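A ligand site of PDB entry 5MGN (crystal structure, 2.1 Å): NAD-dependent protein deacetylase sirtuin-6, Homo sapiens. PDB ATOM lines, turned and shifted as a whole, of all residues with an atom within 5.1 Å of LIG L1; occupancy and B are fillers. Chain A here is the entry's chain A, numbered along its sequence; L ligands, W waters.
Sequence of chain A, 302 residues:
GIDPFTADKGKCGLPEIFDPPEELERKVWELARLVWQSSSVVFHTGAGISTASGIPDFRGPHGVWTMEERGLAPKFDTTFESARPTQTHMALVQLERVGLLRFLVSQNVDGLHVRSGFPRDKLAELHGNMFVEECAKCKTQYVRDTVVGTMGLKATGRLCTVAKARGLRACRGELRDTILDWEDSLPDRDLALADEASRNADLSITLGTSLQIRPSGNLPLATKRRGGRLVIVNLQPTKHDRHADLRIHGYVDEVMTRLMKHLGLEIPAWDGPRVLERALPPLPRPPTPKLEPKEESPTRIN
Water W1 lies within hydrogen-bond range of an oxygen (O10) of LIG L1 (2.6 Å), the side-chain amide oxygen of Asn 108 (3.0 Å) and the backbone carbonyl oxygen of Gln 107 (3.0 Å).
Water W3 lies within hydrogen-bond range of the side-chain carboxylate of Glu 16 (2.5 Å) and an oxygen (O4) of LIG L1 (2.7 Å).
Water W5 lies within hydrogen-bond range of the side-chain hydroxyl (OG) of Ser 210 (2.7 Å), an oxygen (O6) of LIG L1 (2.8 Å), the guanidinium group (NH1) of Arg 59 (3.1 Å) and the backbone NH (N) of Gln 212 (3.2 Å).
Water W4 lies within hydrogen-bond range of the backbone carbonyl oxygen (O) of Gly 48, the side-chain hydroxyl (OG1) of Thr 51 and a nitrogen (N3) of LIG L1.
An oxygen (O8) of LIG L1 is in hydrogen-bond range of the side-chain amide nitrogen (ND2) of Asn 234 (2.9 Å).
The side-chain hydroxyl of Thr 51 lies within hydrogen-bond range of a nitrogen (N4) of LIG L1, at 2.9 Å.
The backbone NH (N) of Val 252 lies within hydrogen-bond range of a nitrogen (N1) of LIG L1 (2.9 Å).
A nitrogen (N2) of LIG L1 sits at hydrogen-bond distance from the backbone NH (N) of Leu 235 (3.4 Å).
An oxygen (O10) of LIG L1 sits at hydrogen-bond distance from the backbone carbonyl oxygen (O) of Gln 107, at 2.7 Å.
O6 of LIG L1 sits at hydrogen-bond distance from OG1 of Thr 209, at 2.6 Å.
O10 of LIG L1 is in hydrogen-bond range of ND1 of His 127.
An oxygen (O1) of LIG L1 lies within hydrogen-bond range of the side-chain hydroxyl of Ser 210 (2.5 Å).
N of Gln 236 sits at hydrogen-bond distance from O4 of LIG L1, at 3.1 Å.
An oxygen (O8) of LIG L1 is in hydrogen-bond range of the side-chain amide oxygen (OE1) of Gln 236 (2.6 Å).
An oxygen (O2) of LIG L1 lies within hydrogen-bond range of the backbone NH (N) of Ala 47 (2.9 Å).
NH1 of Arg 59 is in salt-bridge range of O1 of LIG L1 (2.7 Å).
N of Phe 58 is in hydrogen-bond range of O5 of LIG L1.
N of Arg 59 is in hydrogen-bond range of O5 of LIG L1 (2.8 Å).
The backbone NH (N) of Ser 210 lies within hydrogen-bond range of an oxygen (O6) of LIG L1 (3.2 Å).
O of Val 233 sits at hydrogen-bond distance from N of Gly 208 (3.1 Å).
OG of Ser 210 is in hydrogen-bond range of NE2 of Gln 212, 3.4 Å away.
The side-chain amide nitrogen (ND2) of Asn 108 sits at hydrogen-bond distance from the backbone carbonyl oxygen (O) of Gly 46, 3.1 Å away.
OG1 of Thr 209 is in hydrogen-bond range of N of Leu 211.
NE2 of Gln 107 sits at hydrogen-bond distance from OG1 of Thr 209 (3.2 Å).
O of Arg 59 is in hydrogen-bond range of NE2 of Gln 236 (3.0 Å).
The side-chain amide nitrogen (ND2) of Asn 234 lies within hydrogen-bond range of the backbone carbonyl oxygen (O) of Gln 236 (2.8 Å).
A ring nitrogen (ND1) of His 127 is in hydrogen-bond range of the backbone carbonyl oxygen of Gln 107 (3.1 Å).
A nitrogen (N4) of LIG L1 lies close to the backbone carbonyl oxygen (O) of Gly 48.
Merely in contact with LIG L1: Gly 46 (3.2 Å), Asp 57 (3.3 Å), Trp 65 (3.5 Å), Trp 182 (3.7 Å), Gly 208 (3.3 Å), Ile 213 (3.4 Å), Gly 250 (3.3 Å) and Tyr 251 (3.5 Å).
Within 4 Å of LIG L1: Gly 46, Ala 47, Gly 48, Thr 51, Asp 57, Phe 58, Arg 59, Trp 65, Gln 107, His 127, Trp 182, Gly 208, Thr 209, Ser 210, Ile 213, Asn 234, Leu 235, Gln 236, Gly 250, Tyr 251 and Val 252.
The nearest printed residue that does not touch LIG L1 is Leu 211 (4.1 Å).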
ATOM      1  N   GLU A  16     -28.899  18.610 -13.506  1.00  0.00           N
ATOM      2  CA  GLU A  16     -30.304  18.229 -13.207  1.00  0.00           C
ATOM      3  C   GLU A  16     -31.233  19.254 -13.835  1.00  0.00           C
ATOM      4  O   GLU A  16     -30.849  20.413 -13.923  1.00  0.00           O
ATOM      5  CB  GLU A  16     -30.543  18.188 -11.740  1.00  0.00           C
ATOM      6  CG  GLU A  16     -29.617  17.205 -10.972  1.00  0.00           C
ATOM      7  CD  GLU A  16     -30.034  17.148  -9.544  1.00  0.00           C
ATOM      8  OE1 GLU A  16     -30.324  18.254  -9.070  1.00  0.00           O
ATOM      9  OE2 GLU A  16     -30.116  16.036  -8.926  1.00  0.00           O
ATOM     10  N   GLY A  46     -34.407   2.423 -11.107  1.00  0.00           N
ATOM     11  CA  GLY A  46     -32.961   2.554 -10.887  1.00  0.00           C
ATOM     12  C   GLY A  46     -32.713   3.307  -9.609  1.00  0.00           C
ATOM     13  O   GLY A  46     -33.683   3.618  -8.834  1.00  0.00           O
ATOM     14  N   ALA A  47     -31.423   3.582  -9.385  1.00  0.00           N
ATOM     15  CA  ALA A  47     -30.905   4.093  -8.107  1.00  0.00           C
ATOM     16  C   ALA A  47     -31.505   5.360  -7.586  1.00  0.00           C
ATOM     17  O   ALA A  47     -31.571   5.524  -6.347  1.00  0.00           O
ATOM     18  CB  ALA A  47     -29.369   4.181  -8.117  1.00  0.00           C
ATOM     19  N   GLY A  48     -32.118   6.157  -8.461  1.00  0.00           N
ATOM     20  CA  GLY A  48     -32.720   7.389  -8.059  1.00  0.00           C
ATOM     21  C   GLY A  48     -34.007   7.291  -7.260  1.00  0.00           C
ATOM     22  O   GLY A  48     -34.369   8.234  -6.621  1.00  0.00           O
ATOM     23  N   THR A  51     -32.488   7.309  -3.347  1.00  0.00           N
ATOM     24  CA  THR A  51     -31.770   8.479  -2.841  1.00  0.00           C
ATOM     25  C   THR A  51     -32.494   9.168  -1.635  1.00  0.00           C
ATOM     26  O   THR A  51     -31.851   9.603  -0.747  1.00  0.00           O
ATOM     27  CB  THR A  51     -31.411   9.469  -3.974  1.00  0.00           C
ATOM     28  OG1 THR A  51     -32.569   9.977  -4.636  1.00  0.00           O
ATOM     29  CG2 THR A  51     -30.476   8.810  -4.973  1.00  0.00           C
ATOM     30  N   ASP A  57     -26.990   7.541  -5.508  1.00  0.00           N
ATOM     31  CA  ASP A  57     -27.073   6.880  -6.836  1.00  0.00           C
ATOM     32  C   ASP A  57     -25.646   6.695  -7.395  1.00  0.00           C
ATOM     33  O   ASP A  57     -24.617   6.922  -6.685  1.00  0.00           O
ATOM     34  CB  ASP A  57     -28.057   7.661  -7.734  1.00  0.00           C
ATOM     35  CG  ASP A  57     -27.663   9.187  -7.951  1.00  0.00           C
ATOM     36  OD1 ASP A  57     -26.490   9.624  -7.792  1.00  0.00           O
ATOM     37  OD2 ASP A  57     -28.521   9.970  -8.356  1.00  0.00           O
ATOM     38  N   PHE A  58     -25.551   6.267  -8.658  1.00  0.00           N
ATOM     39  CA  PHE A  58     -24.267   6.186  -9.313  1.00  0.00           C
ATOM     40  C   PHE A  58     -23.752   7.486 -10.068  1.00  0.00           C
ATOM     41  O   PHE A  58     -22.527   7.769 -10.092  1.00  0.00           O
ATOM     42  CB  PHE A  58     -24.358   4.929 -10.305  1.00  0.00           C
ATOM     43  CG  PHE A  58     -24.538   3.644  -9.584  1.00  0.00           C
ATOM     44  CD1 PHE A  58     -23.457   3.010  -9.029  1.00  0.00           C
ATOM     45  CD2 PHE A  58     -25.832   3.124  -9.282  1.00  0.00           C
ATOM     46  CE1 PHE A  58     -23.617   1.830  -8.310  1.00  0.00           C
ATOM     47  CE2 PHE A  58     -25.956   1.889  -8.647  1.00  0.00           C
ATOM     48  CZ  PHE A  58     -24.839   1.263  -8.125  1.00  0.00           C
ATOM     49  N   ARG A  59     -24.632   8.155 -10.824  1.00  0.00           N
ATOM     50  CA  ARG A  59     -24.247   9.141 -11.814  1.00  0.00           C
ATOM     51  C   ARG A  59     -24.919  10.442 -11.594  1.00  0.00           C
ATOM     52  O   ARG A  59     -24.770  11.303 -12.424  1.00  0.00           O
ATOM     53  CB  ARG A  59     -24.547   8.680 -13.264  1.00  0.00           C
ATOM     54  CG  ARG A  59     -23.899   7.324 -13.558  1.00  0.00           C
ATOM     55  CD  ARG A  59     -24.096   6.774 -14.971  1.00  0.00           C
ATOM     56  NE  ARG A  59     -23.483   5.468 -15.121  1.00  0.00           N
ATOM     57  CZ  ARG A  59     -24.042   4.285 -14.772  1.00  0.00           C
ATOM     58  NH1 ARG A  59     -25.253   4.225 -14.253  1.00  0.00           N
ATOM     59  NH2 ARG A  59     -23.410   3.105 -14.902  1.00  0.00           N
ATOM     60  N   GLY A  60     -25.563  10.629 -10.443  1.00  0.00           N
ATOM     61  CA  GLY A  60     -26.109  11.978 -10.039  1.00  0.00           C
ATOM     62  C   GLY A  60     -24.984  12.880  -9.568  1.00  0.00           C
ATOM     63  O   GLY A  60     -23.806  12.428  -9.513  1.00  0.00           O
ATOM     64  N   TRP A  65     -20.101   6.940  -8.830  1.00  0.00           N
ATOM     65  CA  TRP A  65     -19.135   7.134  -9.951  1.00  0.00           C
ATOM     66  C   TRP A  65     -18.770   8.622 -10.148  1.00  0.00           C
ATOM     67  O   TRP A  65     -17.577   8.993 -10.258  1.00  0.00           O
ATOM     68  CB  TRP A  65     -19.584   6.534 -11.279  1.00  0.00           C
ATOM     69  CG  TRP A  65     -20.092   5.068 -11.349  1.00  0.00           C
ATOM     70  CD1 TRP A  65     -21.042   4.612 -12.223  1.00  0.00           C
ATOM     71  CD2 TRP A  65     -19.676   3.923 -10.612  1.00  0.00           C
ATOM     72  NE1 TRP A  65     -21.260   3.288 -12.091  1.00  0.00           N
ATOM     73  CE2 TRP A  65     -20.448   2.824 -11.093  1.00  0.00           C
ATOM     74  CE3 TRP A  65     -18.722   3.699  -9.598  1.00  0.00           C
ATOM     75  CZ2 TRP A  65     -20.323   1.563 -10.596  1.00  0.00           C
ATOM     76  CZ3 TRP A  65     -18.623   2.428  -9.066  1.00  0.00           C
ATOM     77  CH2 TRP A  65     -19.424   1.360  -9.565  1.00  0.00           C
ATOM     78  N   GLN A 107     -32.898  -2.336 -11.672  1.00  0.00           N
ATOM     79  CA  GLN A 107     -31.498  -2.451 -11.718  1.00  0.00           C
ATOM     80  C   GLN A 107     -30.858  -2.420 -10.346  1.00  0.00           C
ATOM     81  O   GLN A 107     -29.638  -2.447 -10.239  1.00  0.00           O
ATOM     82  CB  GLN A 107     -30.960  -1.283 -12.553  1.00  0.00           C
ATOM     83  CG  GLN A 107     -31.303  -1.545 -14.059  1.00  0.00           C
ATOM     84  CD  GLN A 107     -30.974  -0.398 -14.943  1.00  0.00           C
ATOM     85  OE1 GLN A 107     -29.796  -0.245 -15.414  1.00  0.00           O
ATOM     86  NE2 GLN A 107     -32.010   0.418 -15.253  1.00  0.00           N
ATOM     87  N   ASN A 108     -31.650  -2.133  -9.314  1.00  0.00           N
ATOM     88  CA  ASN A 108     -31.092  -1.841  -7.989  1.00  0.00           C
ATOM     89  C   ASN A 108     -30.793  -3.119  -7.313  1.00  0.00           C
ATOM     90  O   ASN A 108     -31.630  -4.038  -7.333  1.00  0.00           O
ATOM     91  CB  ASN A 108     -32.150  -1.072  -7.147  1.00  0.00           C
ATOM     92  CG  ASN A 108     -32.517   0.292  -7.744  1.00  0.00           C
ATOM     93  OD1 ASN A 108     -31.784   0.817  -8.546  1.00  0.00           O
ATOM     94  ND2 ASN A 108     -33.610   0.895  -7.285  1.00  0.00           N
ATOM     95  N   HIS A 127     -29.707  -6.999 -11.620  1.00  0.00           N
ATOM     96  CA  HIS A 127     -28.334  -6.865 -11.283  1.00  0.00           C
ATOM     97  C   HIS A 127     -28.089  -7.561  -9.961  1.00  0.00           C
ATOM     98  O   HIS A 127     -27.044  -7.364  -9.387  1.00  0.00           O
ATOM     99  CB  HIS A 127     -27.942  -5.410 -11.238  1.00  0.00           C
ATOM    100  CG  HIS A 127     -28.084  -4.720 -12.547  1.00  0.00           C
ATOM    101  ND1 HIS A 127     -28.030  -3.352 -12.677  1.00  0.00           N
ATOM    102  CD2 HIS A 127     -28.236  -5.206 -13.811  1.00  0.00           C
ATOM    103  CE1 HIS A 127     -28.164  -3.021 -13.933  1.00  0.00           C
ATOM    104  NE2 HIS A 127     -28.298  -4.127 -14.642  1.00  0.00           N
ATOM    105  N   TRP A 182     -18.894  -6.482 -13.299  1.00  0.00           N
ATOM    106  CA  TRP A 182     -18.852  -5.934 -14.655  1.00  0.00           C
ATOM    107  C   TRP A 182     -18.866  -7.048 -15.682  1.00  0.00           C
ATOM    108  O   TRP A 182     -19.544  -6.877 -16.681  1.00  0.00           O
ATOM    109  CB  TRP A 182     -17.643  -5.013 -14.820  1.00  0.00           C
ATOM    110  CG  TRP A 182     -17.749  -3.669 -13.980  1.00  0.00           C
ATOM    111  CD1 TRP A 182     -17.065  -3.355 -12.807  1.00  0.00           C
ATOM    112  CD2 TRP A 182     -18.580  -2.526 -14.285  1.00  0.00           C
ATOM    113  NE1 TRP A 182     -17.415  -2.068 -12.386  1.00  0.00           N
ATOM    114  CE2 TRP A 182     -18.356  -1.564 -13.265  1.00  0.00           C
ATOM    115  CE3 TRP A 182     -19.504  -2.221 -15.319  1.00  0.00           C
ATOM    116  CZ2 TRP A 182     -19.009  -0.317 -13.270  1.00  0.00           C
ATOM    117  CZ3 TRP A 182     -20.130  -0.966 -15.330  1.00  0.00           C
ATOM    118  CH2 TRP A 182     -19.881  -0.039 -14.316  1.00  0.00           C
ATOM    119  N   GLY A 208     -36.179   7.293 -11.929  1.00  0.00           N
ATOM    120  CA  GLY A 208     -34.771   7.270 -11.383  1.00  0.00           C
ATOM    121  C   GLY A 208     -33.754   6.312 -12.020  1.00  0.00           C
ATOM    122  O   GLY A 208     -32.934   5.685 -11.308  1.00  0.00           O
ATOM    123  N   THR A 209     -33.805   6.171 -13.344  1.00  0.00           N
ATOM    124  CA  THR A 209     -32.690   5.621 -14.103  1.00  0.00           C
ATOM    125  C   THR A 209     -32.280   6.517 -15.337  1.00  0.00           C
ATOM    126  O   THR A 209     -33.117   7.122 -15.987  1.00  0.00           O
ATOM    127  CB  THR A 209     -32.885   4.146 -14.477  1.00  0.00           C
ATOM    128  OG1 THR A 209     -31.794   3.623 -15.304  1.00  0.00           O
ATOM    129  CG2 THR A 209     -34.198   3.952 -15.196  1.00  0.00           C
ATOM    130  N   SER A 210     -30.938   6.585 -15.563  1.00  0.00           N
ATOM    131  CA  SER A 210     -30.322   7.290 -16.574  1.00  0.00           C
ATOM    132  C   SER A 210     -30.239   6.397 -17.848  1.00  0.00           C
ATOM    133  O   SER A 210     -29.962   6.940 -18.905  1.00  0.00           O
ATOM    134  CB  SER A 210     -28.966   7.855 -16.137  1.00  0.00           C
ATOM    135  OG  SER A 210     -28.037   6.883 -15.809  1.00  0.00           O
ATOM    136  N   LEU A 211     -30.712   5.152 -17.767  1.00  0.00           N
ATOM    137  CA  LEU A 211     -30.867   4.258 -18.959  1.00  0.00           C
ATOM    138  C   LEU A 211     -29.591   3.950 -19.786  1.00  0.00           C
ATOM    139  O   LEU A 211     -29.651   3.456 -20.883  1.00  0.00           O
ATOM    140  CB  LEU A 211     -32.047   4.793 -19.883  1.00  0.00           C
ATOM    141  CG  LEU A 211     -33.347   4.778 -19.164  1.00  0.00           C
ATOM    142  CD1 LEU A 211     -34.467   5.418 -20.047  1.00  0.00           C
ATOM    143  CD2 LEU A 211     -33.746   3.369 -18.741  1.00  0.00           C
ATOM    144  N   GLN A 212     -28.429   4.052 -19.154  1.00  0.00           N
ATOM    145  CA  GLN A 212     -27.197   3.918 -19.804  1.00  0.00           C
ATOM    146  C   GLN A 212     -26.658   2.485 -19.850  1.00  0.00           C
ATOM    147  O   GLN A 212     -25.777   2.249 -20.620  1.00  0.00           O
ATOM    148  CB  GLN A 212     -26.152   4.840 -19.121  1.00  0.00           C
ATOM    149  CG  GLN A 212     -26.401   6.325 -19.231  1.00  0.00           C
ATOM    150  CD  GLN A 212     -25.245   7.139 -18.672  1.00  0.00           C
ATOM    151  OE1 GLN A 212     -24.140   7.013 -19.172  1.00  0.00           O
ATOM    152  NE2 GLN A 212     -25.489   8.003 -17.685  1.00  0.00           N
ATOM    153  N   ILE A 213     -27.117   1.559 -19.007  1.00  0.00           N
ATOM    154  CA  ILE A 213     -26.641   0.205 -18.994  1.00  0.00           C
ATOM    155  C   ILE A 213     -27.409  -0.668 -19.956  1.00  0.00           C
ATOM    156  O   ILE A 213     -28.615  -0.581 -20.021  1.00  0.00           O
ATOM    157  CB  ILE A 213     -26.714  -0.372 -17.543  1.00  0.00           C
ATOM    158  CG1 ILE A 213     -25.539   0.159 -16.712  1.00  0.00           C
ATOM    159  CG2 ILE A 213     -26.662  -1.915 -17.516  1.00  0.00           C
ATOM    160  CD1 ILE A 213     -24.150  -0.450 -17.077  1.00  0.00           C
ATOM    161  N   VAL A 233     -39.309   9.439 -16.012  1.00  0.00           N
ATOM    162  CA  VAL A 233     -39.285  10.437 -14.860  1.00  0.00           C
ATOM    163  C   VAL A 233     -37.870  10.384 -14.326  1.00  0.00           C
ATOM    164  O   VAL A 233     -37.421   9.325 -13.863  1.00  0.00           O
ATOM    165  CB  VAL A 233     -40.233  10.024 -13.722  1.00  0.00           C
ATOM    166  CG1 VAL A 233     -40.228  11.026 -12.546  1.00  0.00           C
ATOM    167  CG2 VAL A 233     -41.653   9.864 -14.232  1.00  0.00           C
ATOM    168  N   ASN A 234     -37.151  11.547 -14.395  1.00  0.00           N
ATOM    169  CA  ASN A 234     -35.737  11.597 -14.058  1.00  0.00           C
ATOM    170  C   ASN A 234     -35.291  13.100 -13.875  1.00  0.00           C
ATOM    171  O   ASN A 234     -35.692  14.008 -14.634  1.00  0.00           O
ATOM    172  CB  ASN A 234     -34.852  10.825 -15.132  1.00  0.00           C
ATOM    173  CG  ASN A 234     -33.570  10.274 -14.546  1.00  0.00           C
ATOM    174  OD1 ASN A 234     -33.629   9.407 -13.663  1.00  0.00           O
ATOM    175  ND2 ASN A 234     -32.354  10.833 -14.974  1.00  0.00           N
ATOM    176  N   LEU A 235     -34.478  13.376 -12.851  1.00  0.00           N
ATOM    177  CA  LEU A 235     -33.862  14.651 -12.688  1.00  0.00           C
ATOM    178  C   LEU A 235     -32.824  14.994 -13.794  1.00  0.00           C
ATOM    179  O   LEU A 235     -32.864  16.038 -14.340  1.00  0.00           O
ATOM    180  CB  LEU A 235     -33.236  14.766 -11.300  1.00  0.00           C
ATOM    181  CG  LEU A 235     -34.355  15.056 -10.306  1.00  0.00           C
ATOM    182  CD1 LEU A 235     -33.832  14.793  -8.910  1.00  0.00           C
ATOM    183  CD2 LEU A 235     -34.782  16.511 -10.372  1.00  0.00           C
ATOM    184  N   GLN A 236     -31.967  14.052 -14.180  1.00  0.00           N
ATOM    185  CA  GLN A 236     -31.006  14.249 -15.220  1.00  0.00           C
ATOM    186  C   GLN A 236     -31.546  13.814 -16.559  1.00  0.00           C
ATOM    187  O   GLN A 236     -32.573  13.091 -16.655  1.00  0.00           O
ATOM    188  CB  GLN A 236     -29.706  13.456 -14.984  1.00  0.00           C
ATOM    189  CG  GLN A 236     -28.782  13.954 -13.902  1.00  0.00           C
ATOM    190  CD  GLN A 236     -27.614  13.034 -13.649  1.00  0.00           C
ATOM    191  OE1 GLN A 236     -27.723  11.803 -13.780  1.00  0.00           O
ATOM    192  NE2 GLN A 236     -26.451  13.613 -13.310  1.00  0.00           N
ATOM    193  N   PRO A 237     -30.869  14.266 -17.642  1.00  0.00           N
ATOM    194  CA  PRO A 237     -31.046  13.598 -18.927  1.00  0.00           C
ATOM    195  C   PRO A 237     -30.723  12.073 -18.844  1.00  0.00           C
ATOM    196  O   PRO A 237     -29.804  11.662 -18.139  1.00  0.00           O
ATOM    197  CB  PRO A 237     -30.126  14.384 -19.856  1.00  0.00           C
ATOM    198  CG  PRO A 237     -29.542  15.519 -19.089  1.00  0.00           C
ATOM    199  CD  PRO A 237     -29.934  15.413 -17.681  1.00  0.00           C
ATOM    200  N   GLY A 250     -38.482  15.953 -12.245  1.00  0.00           N
ATOM    201  CA  GLY A 250     -38.880  16.255 -10.884  1.00  0.00           C
ATOM    202  C   GLY A 250     -38.422  15.203  -9.968  1.00  0.00           C
ATOM    203  O   GLY A 250     -37.983  14.144 -10.421  1.00  0.00           O
ATOM    204  N   TYR A 251     -38.490  15.480  -8.657  1.00  0.00           N
ATOM    205  CA  TYR A 251     -38.305  14.417  -7.694  1.00  0.00           C
ATOM    206  C   TYR A 251     -39.341  13.322  -7.795  1.00  0.00           C
ATOM    207  O   TYR A 251     -40.565  13.630  -7.811  1.00  0.00           O
ATOM    208  CB  TYR A 251     -38.347  14.973  -6.288  1.00  0.00           C
ATOM    209  CG  TYR A 251     -37.212  15.894  -6.083  1.00  0.00           C
ATOM    210  CD1 TYR A 251     -35.947  15.401  -5.901  1.00  0.00           C
ATOM    211  CD2 TYR A 251     -37.411  17.280  -6.136  1.00  0.00           C
ATOM    212  CE1 TYR A 251     -34.870  16.236  -5.729  1.00  0.00           C
ATOM    213  CE2 TYR A 251     -36.326  18.145  -5.992  1.00  0.00           C
ATOM    214  CZ  TYR A 251     -35.073  17.607  -5.753  1.00  0.00           C
ATOM    215  OH  TYR A 251     -34.004  18.438  -5.592  1.00  0.00           O
ATOM    216  N   VAL A 252     -38.888  12.056  -7.896  1.00  0.00           N
ATOM    217  CA  VAL A 252     -39.808  10.977  -8.032  1.00  0.00           C
ATOM    218  C   VAL A 252     -40.852  10.812  -6.916  1.00  0.00           C
ATOM    219  O   VAL A 252     -42.014  10.590  -7.238  1.00  0.00           O
ATOM    220  CB  VAL A 252     -39.200   9.612  -8.250  1.00  0.00           C
ATOM    221  CG1 VAL A 252     -38.624   9.628  -9.600  1.00  0.00           C
ATOM    222  CG2 VAL A 252     -38.204   9.129  -7.165  1.00  0.00           C
HETATM  223  N1  LIG L   1     -35.991  11.853  -8.397  1.00  0.00           N
HETATM  224  C1  LIG L   1     -35.802  11.734  -9.699  1.00  0.00           C
HETATM  225  N2  LIG L   1     -34.667  11.342 -10.191  1.00  0.00           N
HETATM  226  C2  LIG L   1     -33.637  11.078  -9.398  1.00  0.00           C
HETATM  227  C3  LIG L   1     -33.721  11.225  -7.963  1.00  0.00           C
HETATM  228  C4  LIG L   1     -34.995  11.625  -7.474  1.00  0.00           C
HETATM  229  N3  LIG L   1     -35.140  11.742  -6.111  1.00  0.00           N
HETATM  230  N4  LIG L   1     -32.546  10.904  -7.411  1.00  0.00           N
HETATM  231  C5  LIG L   1     -31.750  10.548  -8.417  1.00  0.00           C
HETATM  232  N5  LIG L   1     -32.412  10.715  -9.621  1.00  0.00           N
HETATM  233  P1  LIG L   1     -27.877   6.229 -12.258  1.00  0.00           P
HETATM  234  P2  LIG L   1     -29.044   3.544 -12.603  1.00  0.00           P
HETATM  235  C6  LIG L   1     -31.898  10.400 -10.949  1.00  0.00           C
HETATM  236  O1  LIG L   1     -27.089   6.063 -13.614  1.00  0.00           O
HETATM  237  O2  LIG L   1     -29.826   2.696 -11.648  1.00  0.00           O
HETATM  238  C7  LIG L   1     -24.546   0.891 -12.327  1.00  0.00           C
HETATM  239  O3  LIG L   1     -23.215   0.427 -12.751  1.00  0.00           O
HETATM  240  C8  LIG L   1     -30.516  10.949 -11.356  1.00  0.00           C
HETATM  241  O4  LIG L   1     -30.723  12.255 -11.957  1.00  0.00           O
HETATM  242  O5  LIG L   1     -27.071   6.813 -11.113  1.00  0.00           O
HETATM  243  O6  LIG L   1     -29.621   4.096 -13.948  1.00  0.00           O
HETATM  244  C9  LIG L   1     -25.304  -0.129 -11.495  1.00  0.00           C
HETATM  245  O7  LIG L   1     -24.995  -1.360 -12.222  1.00  0.00           O
HETATM  246  C10 LIG L   1     -29.900   9.850 -12.189  1.00  0.00           C
HETATM  247  O8  LIG L   1     -29.887  10.413 -13.450  1.00  0.00           O
HETATM  248  O9  LIG L   1     -28.316   4.737 -11.854  1.00  0.00           O
HETATM  249  C11 LIG L   1     -26.790   0.185 -11.728  1.00  0.00           C
HETATM  250  O10 LIG L   1     -27.639  -1.023 -11.389  1.00  0.00           O
HETATM  251  C12 LIG L   1     -30.761   8.631 -11.951  1.00  0.00           C
HETATM  252  O11 LIG L   1     -31.629   9.036 -10.858  1.00  0.00           O
HETATM  253  C13 LIG L   1     -26.700   0.547 -13.221  1.00  0.00           C
HETATM  254  O12 LIG L   1     -25.409   1.109 -13.481  1.00  0.00           O
HETATM  255  C14 LIG L   1     -30.137   7.335 -11.498  1.00  0.00           C
HETATM  256  O13 LIG L   1     -29.248   6.862 -12.553  1.00  0.00           O
HETATM  257  C15 LIG L   1     -27.696   1.549 -13.708  1.00  0.00           C
HETATM  258  O14 LIG L   1     -27.727   2.679 -12.824  1.00  0.00           O
HETATM  259  N1  LG2 L   2     -22.803  -2.427  -5.143  1.00  0.00           N
HETATM  260  C1  LG2 L   2     -22.843  -1.338  -5.996  1.00  0.00           C
HETATM  261  C2  LG2 L   2     -23.128  -1.765  -7.270  1.00  0.00           C
HETATM  262  C3  LG2 L   2     -23.273  -3.176  -7.231  1.00  0.00           C
HETATM  263  C4  LG2 L   2     -23.046  -3.575  -5.889  1.00  0.00           C
HETATM  264  C5  LG2 L   2     -22.502  -2.269  -3.762  1.00  0.00           C
HETATM  265  C6  LG2 L   2     -22.862  -3.208  -2.802  1.00  0.00           C
HETATM  266  C7  LG2 L   2     -22.548  -2.961  -1.478  1.00  0.00           C
HETATM  267  C8  LG2 L   2     -21.872  -1.814  -1.091  1.00  0.00           C
HETATM  268  C9  LG2 L   2     -21.527  -0.859  -2.026  1.00  0.00           C
HETATM  269  C10 LG2 L   2     -21.797  -1.094  -3.373  1.00  0.00           C
HETATM  270  N2  LG2 L   2     -21.514  -0.129  -4.405  1.00  0.00           N
HETATM  271  C11 LG2 L   2     -23.863   0.631  -4.845  1.00  0.00           C
HETATM  272  C12 LG2 L   2     -26.218   0.609  -4.356  1.00  0.00           C
HETATM  273  C13 LG2 L   2     -25.077  -0.045  -4.805  1.00  0.00           C
HETATM  274  C14 LG2 L   2     -23.874   1.948  -4.361  1.00  0.00           C
HETATM  275  N3  LG2 L   2     -24.964   2.578  -3.887  1.00  0.00           N
HETATM  276  C15 LG2 L   2     -26.112   1.920  -3.928  1.00  0.00           C
HETATM  277  C16 LG2 L   2     -22.599  -0.032  -5.402  1.00  0.00           C
HETATM  278  S1  LG2 L   2     -19.911   0.335  -4.854  1.00  0.00           S
HETATM  279  O1  LG2 L   2     -20.039   1.651  -5.390  1.00  0.00           O
HETATM  280  O2  LG2 L   2     -19.116   0.134  -3.679  1.00  0.00           O
HETATM  281  C17 LG2 L   2     -19.215  -0.702  -6.116  1.00  0.00           C
HETATM  282  C18 LG2 L   2     -19.760  -1.960  -6.374  1.00  0.00           C
HETATM  283  C19 LG2 L   2     -19.179  -2.769  -7.336  1.00  0.00           C
HETATM  284  C20 LG2 L   2     -18.050  -2.358  -8.015  1.00  0.00           C
HETATM  285  C21 LG2 L   2     -17.478  -1.115  -7.755  1.00  0.00           C
HETATM  286  C22 LG2 L   2     -18.042  -0.291  -6.765  1.00  0.00           C
HETATM  287  C23 LG2 L   2     -16.247  -0.682  -8.519  1.00  0.00           C
HETATM  288  F1  LG2 L   2     -16.367   0.512  -9.117  1.00  0.00           F
HETATM  289  F2  LG2 L   2     -15.879  -1.583  -9.545  1.00  0.00           F
HETATM  290  F3  LG2 L   2     -15.175  -0.599  -7.709  1.00  0.00           F
HETATM  291  O   HOH W   1     -29.156   0.538  -9.977  1.00  0.00           O
HETATM  292  O   HOH W   2     -37.725  11.301  -4.625  1.00  0.00           O
HETATM  293  O   HOH W   3     -29.779  13.690  -9.858  1.00  0.00           O
HETATM  294  O   HOH W   4     -35.628   8.977  -4.060  1.00  0.00           O
HETATM  295  O   HOH W   5     -27.741   4.206 -16.024  1.00  0.00           O
